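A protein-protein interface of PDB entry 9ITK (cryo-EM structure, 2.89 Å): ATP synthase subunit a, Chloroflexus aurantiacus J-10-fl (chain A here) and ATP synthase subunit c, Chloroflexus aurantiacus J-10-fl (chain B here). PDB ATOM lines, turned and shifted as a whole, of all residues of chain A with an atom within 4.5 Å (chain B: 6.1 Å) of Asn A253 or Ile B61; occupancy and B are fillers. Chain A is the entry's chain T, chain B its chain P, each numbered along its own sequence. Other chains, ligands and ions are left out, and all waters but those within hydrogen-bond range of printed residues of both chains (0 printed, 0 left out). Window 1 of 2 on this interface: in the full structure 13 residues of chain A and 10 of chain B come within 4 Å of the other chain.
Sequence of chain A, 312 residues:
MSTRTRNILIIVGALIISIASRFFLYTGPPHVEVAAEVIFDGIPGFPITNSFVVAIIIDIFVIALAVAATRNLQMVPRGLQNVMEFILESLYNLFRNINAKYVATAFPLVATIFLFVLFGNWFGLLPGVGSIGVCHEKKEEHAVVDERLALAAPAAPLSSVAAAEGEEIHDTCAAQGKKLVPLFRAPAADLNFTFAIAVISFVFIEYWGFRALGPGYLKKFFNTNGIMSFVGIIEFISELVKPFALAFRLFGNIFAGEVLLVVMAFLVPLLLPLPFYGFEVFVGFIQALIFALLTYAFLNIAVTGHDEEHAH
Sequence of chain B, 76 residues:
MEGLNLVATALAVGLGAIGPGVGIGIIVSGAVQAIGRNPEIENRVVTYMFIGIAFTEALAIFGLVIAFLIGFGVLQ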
ATOM      1  N   ARG A 249      24.992  25.817  11.042  1.00  0.00           N
ATOM      2  CA  ARG A 249      24.462  25.668  12.392  1.00  0.00           C
ATOM      3  C   ARG A 249      25.490  26.075  13.438  1.00  0.00           C
ATOM      4  O   ARG A 249      25.165  26.765  14.410  1.00  0.00           O
ATOM      5  CB  ARG A 249      24.010  24.227  12.616  1.00  0.00           C
ATOM      6  CG  ARG A 249      23.358  23.977  13.960  1.00  0.00           C
ATOM      7  CD  ARG A 249      23.473  22.517  14.359  1.00  0.00           C
ATOM      8  NE  ARG A 249      23.400  21.629  13.205  1.00  0.00           N
ATOM      9  CZ  ARG A 249      22.278  21.310  12.574  1.00  0.00           C
ATOM     10  NH1 ARG A 249      21.108  21.789  12.961  1.00  0.00           N
ATOM     11  NH2 ARG A 249      22.333  20.491  11.528  1.00  0.00           N
ATOM     12  N   LEU A 250      26.742  25.652  13.258  1.00  0.00           N
ATOM     13  CA  LEU A 250      27.772  25.996  14.230  1.00  0.00           C
ATOM     14  C   LEU A 250      28.159  27.465  14.133  1.00  0.00           C
ATOM     15  O   LEU A 250      28.291  28.144  15.158  1.00  0.00           O
ATOM     16  CB  LEU A 250      28.997  25.104  14.042  1.00  0.00           C
ATOM     17  CG  LEU A 250      30.108  25.347  15.060  1.00  0.00           C
ATOM     18  CD1 LEU A 250      29.614  25.035  16.459  1.00  0.00           C
ATOM     19  CD2 LEU A 250      31.323  24.504  14.725  1.00  0.00           C
ATOM     20  N   PHE A 251      28.350  27.974  12.914  1.00  0.00           N
ATOM     21  CA  PHE A 251      28.725  29.375  12.756  1.00  0.00           C
ATOM     22  C   PHE A 251      27.632  30.296  13.275  1.00  0.00           C
ATOM     23  O   PHE A 251      27.907  31.257  14.002  1.00  0.00           O
ATOM     24  CB  PHE A 251      29.019  29.688  11.290  1.00  0.00           C
ATOM     25  CG  PHE A 251      28.980  31.158  10.971  1.00  0.00           C
ATOM     26  CD1 PHE A 251      29.826  32.043  11.616  1.00  0.00           C
ATOM     27  CD2 PHE A 251      28.084  31.655  10.043  1.00  0.00           C
ATOM     28  CE1 PHE A 251      29.788  33.391  11.328  1.00  0.00           C
ATOM     29  CE2 PHE A 251      28.045  33.003   9.753  1.00  0.00           C
ATOM     30  CZ  PHE A 251      28.897  33.871  10.397  1.00  0.00           C
ATOM     31  N   GLY A 252      26.381  30.016  12.910  1.00  0.00           N
ATOM     32  CA  GLY A 252      25.297  30.898  13.302  1.00  0.00           C
ATOM     33  C   GLY A 252      25.112  30.954  14.805  1.00  0.00           C
ATOM     34  O   GLY A 252      24.984  32.032  15.390  1.00  0.00           O
ATOM     35  N   ASN A 253      25.113  29.789  15.453  1.00  0.00           N
ATOM     36  CA  ASN A 253      24.860  29.738  16.886  1.00  0.00           C
ATOM     37  C   ASN A 253      26.005  30.310  17.710  1.00  0.00           C
ATOM     38  O   ASN A 253      25.822  30.543  18.909  1.00  0.00           O
ATOM     39  CB  ASN A 253      24.576  28.300  17.313  1.00  0.00           C
ATOM     40  CG  ASN A 253      23.518  28.218  18.391  1.00  0.00           C
ATOM     41  OD1 ASN A 253      23.379  29.128  19.207  1.00  0.00           O
ATOM     42  ND2 ASN A 253      22.755  27.133  18.390  1.00  0.00           N
ATOM     43  N   ILE A 254      27.169  30.539  17.107  1.00  0.00           N
ATOM     44  CA  ILE A 254      28.274  31.195  17.794  1.00  0.00           C
ATOM     45  C   ILE A 254      28.298  32.661  17.385  1.00  0.00           C
ATOM     46  O   ILE A 254      28.609  33.540  18.197  1.00  0.00           O
ATOM     47  CB  ILE A 254      29.612  30.499  17.494  1.00  0.00           C
ATOM     48  CG1 ILE A 254      29.563  29.052  17.985  1.00  0.00           C
ATOM     49  CG2 ILE A 254      30.763  31.240  18.148  1.00  0.00           C
ATOM     50  CD1 ILE A 254      29.170  28.922  19.439  1.00  0.00           C
ATOM     51  N   PHE A 255      27.961  32.935  16.123  1.00  0.00           N
ATOM     52  CA  PHE A 255      27.782  34.320  15.702  1.00  0.00           C
ATOM     53  C   PHE A 255      26.646  34.974  16.475  1.00  0.00           C
ATOM     54  O   PHE A 255      26.692  36.174  16.767  1.00  0.00           O
ATOM     55  CB  PHE A 255      27.523  34.385  14.198  1.00  0.00           C
ATOM     56  CG  PHE A 255      27.684  35.759  13.612  1.00  0.00           C
ATOM     57  CD1 PHE A 255      26.630  36.654  13.613  1.00  0.00           C
ATOM     58  CD2 PHE A 255      28.886  36.150  13.053  1.00  0.00           C
ATOM     59  CE1 PHE A 255      26.773  37.914  13.071  1.00  0.00           C
ATOM     60  CE2 PHE A 255      29.035  37.410  12.509  1.00  0.00           C
ATOM     61  CZ  PHE A 255      27.976  38.292  12.519  1.00  0.00           C
ATOM     62  N   ALA A 256      25.608  34.202  16.802  1.00  0.00           N
ATOM     63  CA  ALA A 256      24.603  34.688  17.740  1.00  0.00           C
ATOM     64  C   ALA A 256      25.211  34.905  19.119  1.00  0.00           C
ATOM     65  O   ALA A 256      24.909  35.899  19.791  1.00  0.00           O
ATOM     66  CB  ALA A 256      23.433  33.709  17.815  1.00  0.00           C
ATOM     67  N   GLY A 257      26.067  33.982  19.560  1.00  0.00           N
ATOM     68  CA  GLY A 257      26.790  34.194  20.803  1.00  0.00           C
ATOM     69  C   GLY A 257      27.760  35.355  20.711  1.00  0.00           C
ATOM     70  O   GLY A 257      28.036  36.026  21.708  1.00  0.00           O
ATOM     71  N   VAL A 283      24.687  26.700  25.313  1.00  0.00           N
ATOM     72  CA  VAL A 283      24.474  26.399  23.902  1.00  0.00           C
ATOM     73  C   VAL A 283      25.801  26.110  23.210  1.00  0.00           C
ATOM     74  O   VAL A 283      25.875  25.257  22.319  1.00  0.00           O
ATOM     75  CB  VAL A 283      23.695  27.538  23.215  1.00  0.00           C
ATOM     76  CG1 VAL A 283      24.499  28.824  23.200  1.00  0.00           C
ATOM     77  CG2 VAL A 283      23.300  27.134  21.807  1.00  0.00           C
ATOM     78  N   GLN A 287      26.258  22.845  21.060  1.00  0.00           N
ATOM     79  CA  GLN A 287      26.707  22.828  19.670  1.00  0.00           C
ATOM     80  C   GLN A 287      27.966  21.991  19.513  1.00  0.00           C
ATOM     81  O   GLN A 287      28.140  21.296  18.506  1.00  0.00           O
ATOM     82  CB  GLN A 287      26.943  24.252  19.167  1.00  0.00           C
ATOM     83  CG  GLN A 287      25.733  25.170  19.248  1.00  0.00           C
ATOM     84  CD  GLN A 287      24.533  24.644  18.485  1.00  0.00           C
ATOM     85  OE1 GLN A 287      23.388  24.887  18.865  1.00  0.00           O
ATOM     86  NE2 GLN A 287      24.787  23.957  17.378  1.00  0.00           N
ATOM     87  N   GLY B  16      10.652  33.081  11.297  1.00  0.00           N
ATOM     88  CA  GLY B  16      11.742  32.180  11.572  1.00  0.00           C
ATOM     89  C   GLY B  16      11.897  31.829  13.034  1.00  0.00           C
ATOM     90  O   GLY B  16      12.551  30.832  13.352  1.00  0.00           O
ATOM     91  N   ALA B  54      18.515  21.608  19.373  1.00  0.00           N
ATOM     92  CA  ALA B  54      19.532  22.287  18.584  1.00  0.00           C
ATOM     93  C   ALA B  54      19.136  22.378  17.116  1.00  0.00           C
ATOM     94  O   ALA B  54      19.442  23.372  16.449  1.00  0.00           O
ATOM     95  CB  ALA B  54      20.866  21.572  18.742  1.00  0.00           C
ATOM     96  N   THR B  56      15.972  22.643  15.941  1.00  0.00           N
ATOM     97  CA  THR B  56      14.998  23.724  15.862  1.00  0.00           C
ATOM     98  C   THR B  56      15.660  25.075  16.096  1.00  0.00           C
ATOM     99  O   THR B  56      15.416  26.032  15.353  1.00  0.00           O
ATOM    100  CB  THR B  56      13.882  23.496  16.874  1.00  0.00           C
ATOM    101  OG1 THR B  56      14.442  23.458  18.190  1.00  0.00           O
ATOM    102  CG2 THR B  56      13.183  22.181  16.600  1.00  0.00           C
ATOM    103  N   GLU B  57      16.515  25.167  17.117  1.00  0.00           N
ATOM    104  CA  GLU B  57      17.210  26.422  17.381  1.00  0.00           C
ATOM    105  C   GLU B  57      18.113  26.817  16.223  1.00  0.00           C
ATOM    106  O   GLU B  57      18.379  28.006  16.027  1.00  0.00           O
ATOM    107  CB  GLU B  57      18.023  26.314  18.671  1.00  0.00           C
ATOM    108  CG  GLU B  57      17.221  26.567  19.933  1.00  0.00           C
ATOM    109  CD  GLU B  57      17.242  28.022  20.355  1.00  0.00           C
ATOM    110  OE1 GLU B  57      17.378  28.897  19.474  1.00  0.00           O
ATOM    111  OE2 GLU B  57      17.122  28.293  21.567  1.00  0.00           O
ATOM    112  N   ALA B  58      18.587  25.841  15.447  1.00  0.00           N
ATOM    113  CA  ALA B  58      19.454  26.149  14.316  1.00  0.00           C
ATOM    114  C   ALA B  58      18.742  27.035  13.305  1.00  0.00           C
ATOM    115  O   ALA B  58      19.318  28.001  12.793  1.00  0.00           O
ATOM    116  CB  ALA B  58      19.928  24.857  13.651  1.00  0.00           C
ATOM    117  N   LEU B  59      17.481  26.721  13.005  1.00  0.00           N
ATOM    118  CA  LEU B  59      16.743  27.511  12.028  1.00  0.00           C
ATOM    119  C   LEU B  59      16.384  28.880  12.584  1.00  0.00           C
ATOM    120  O   LEU B  59      16.357  29.870  11.844  1.00  0.00           O
ATOM    121  CB  LEU B  59      15.491  26.760  11.593  1.00  0.00           C
ATOM    122  CG  LEU B  59      15.850  25.508  10.803  1.00  0.00           C
ATOM    123  CD1 LEU B  59      14.638  24.615  10.601  1.00  0.00           C
ATOM    124  CD2 LEU B  59      16.493  25.902   9.490  1.00  0.00           C
ATOM    125  N   ALA B  60      16.099  28.955  13.883  1.00  0.00           N
ATOM    126  CA  ALA B  60      15.804  30.243  14.497  1.00  0.00           C
ATOM    127  C   ALA B  60      17.010  31.167  14.444  1.00  0.00           C
ATOM    128  O   ALA B  60      16.873  32.365  14.172  1.00  0.00           O
ATOM    129  CB  ALA B  60      15.352  30.039  15.938  1.00  0.00           C
ATOM    130  N   ILE B  61      18.203  30.630  14.708  1.00  0.00           N
ATOM    131  CA  ILE B  61      19.410  31.446  14.648  1.00  0.00           C
ATOM    132  C   ILE B  61      19.707  31.871  13.216  1.00  0.00           C
ATOM    133  O   ILE B  61      20.212  32.976  12.985  1.00  0.00           O
ATOM    134  CB  ILE B  61      20.593  30.696  15.279  1.00  0.00           C
ATOM    135  CG1 ILE B  61      20.283  30.355  16.735  1.00  0.00           C
ATOM    136  CG2 ILE B  61      21.837  31.540  15.220  1.00  0.00           C
ATOM    137  CD1 ILE B  61      20.041  31.566  17.607  1.00  0.00           C
ATOM    138  N   PHE B  62      19.404  31.014  12.234  1.00  0.00           N
ATOM    139  CA  PHE B  62      19.592  31.402  10.839  1.00  0.00           C
ATOM    140  C   PHE B  62      18.844  32.686  10.513  1.00  0.00           C
ATOM    141  O   PHE B  62      19.283  33.461   9.658  1.00  0.00           O
ATOM    142  CB  PHE B  62      19.136  30.287   9.898  1.00  0.00           C
ATOM    143  CG  PHE B  62      19.985  29.050   9.959  1.00  0.00           C
ATOM    144  CD1 PHE B  62      21.229  29.071  10.560  1.00  0.00           C
ATOM    145  CD2 PHE B  62      19.540  27.867   9.394  1.00  0.00           C
ATOM    146  CE1 PHE B  62      22.006  27.931  10.610  1.00  0.00           C
ATOM    147  CE2 PHE B  62      20.312  26.727   9.440  1.00  0.00           C
ATOM    148  CZ  PHE B  62      21.547  26.759  10.048  1.00  0.00           C
ATOM    149  N   GLY B  63      17.712  32.923  11.175  1.00  0.00           N
ATOM    150  CA  GLY B  63      17.048  34.206  11.039  1.00  0.00           C
ATOM    151  C   GLY B  63      17.850  35.342  11.643  1.00  0.00           C
ATOM    152  O   GLY B  63      17.866  36.453  11.109  1.00  0.00           O
ATOM    153  N   LEU B  64      18.526  35.083  12.766  1.00  0.00           N
ATOM    154  CA  LEU B  64      19.284  36.135  13.436  1.00  0.00           C
ATOM    155  C   LEU B  64      20.491  36.569  12.615  1.00  0.00           C
ATOM    156  O   LEU B  64      20.727  37.768  12.431  1.00  0.00           O
ATOM    157  CB  LEU B  64      19.730  35.670  14.818  1.00  0.00           C
ATOM    158  CG  LEU B  64      18.679  35.708  15.919  1.00  0.00           C
ATOM    159  CD1 LEU B  64      19.274  35.146  17.184  1.00  0.00           C
ATOM    160  CD2 LEU B  64      18.204  37.130  16.134  1.00  0.00           C
ATOM    161  N   VAL B  65      21.277  35.610  12.121  1.00  0.00           N
ATOM    162  CA  VAL B  65      22.466  35.970  11.356  1.00  0.00           C
ATOM    163  C   VAL B  65      22.073  36.740  10.103  1.00  0.00           C
ATOM    164  O   VAL B  65      22.715  37.732   9.740  1.00  0.00           O
ATOM    165  CB  VAL B  65      23.305  34.720  11.027  1.00  0.00           C
ATOM    166  CG1 VAL B  65      23.967  34.192  12.282  1.00  0.00           C
ATOM    167  CG2 VAL B  65      22.450  33.644  10.390  1.00  0.00           C
ATOM    168  N   ILE B  66      20.998  36.314   9.436  1.00  0.00           N
ATOM    169  CA  ILE B  66      20.488  37.074   8.302  1.00  0.00           C
ATOM    170  C   ILE B  66      19.980  38.434   8.759  1.00  0.00           C
ATOM    171  O   ILE B  66      20.125  39.432   8.043  1.00  0.00           O
ATOM    172  CB  ILE B  66      19.397  36.273   7.569  1.00  0.00           C
ATOM    173  CG1 ILE B  66      20.004  35.033   6.915  1.00  0.00           C
ATOM    174  CG2 ILE B  66      18.720  37.131   6.521  1.00  0.00           C
ATOM    175  CD1 ILE B  66      21.003  35.349   5.834  1.00  0.00           C
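Among the printed residues, pairs that only touch across the chains: Gly A252 with Ile B61 (3.2 Å), Arg A249 with Ala B58 (3.4 Å), Arg A249 with Phe B62 (3.7 Å), Gly A252 with Val B65 (3.7 Å), Asn A253 with Ile B61 (3.7 Å), Ala A256 with Ile B61 (3.7 Å) and Phe A255 with Val B65 (3.9 Å).
Printed residues of chain B that touch a printed residue of chain A: Ala B58, Ile B61, Phe B62 and Val B65. Of the 11 printed residues of chain A, 5 touch a printed residue of chain B. Hydrophobic or aromatic side chains of chain A within 4 Å of the printed part of chain B: Phe A255 and Ala A256. Among the printed residues, no Asp or Glu carboxylate lies within 4 Å of a Lys or Arg side-chain nitrogen of the other chain.
Ile B61 touches just these residues of chain A: Gly A252 (3.2 Å), Asn A253 (3.7 Å) and Ala A256 (3.7 Å). Of the printed residues of chain B, Ala A256 touches Ile B61 (3.7 Å). Printed residues of chain B within 4 Å of Phe A255: Val B65 (3.9 Å). Of the printed residues of chain B, Arg A249 touches Ala B58 (3.4 Å) and Phe B62 (3.7 Å). Ile A254 touches none of the printed residues of chain B. The nearest residue of chain B that does not touch Asn A253 is Glu B57 (4.8 Å). The nearest printed residue of chain B that does not touch Phe A255 is Ile B61 (6.0 Å).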
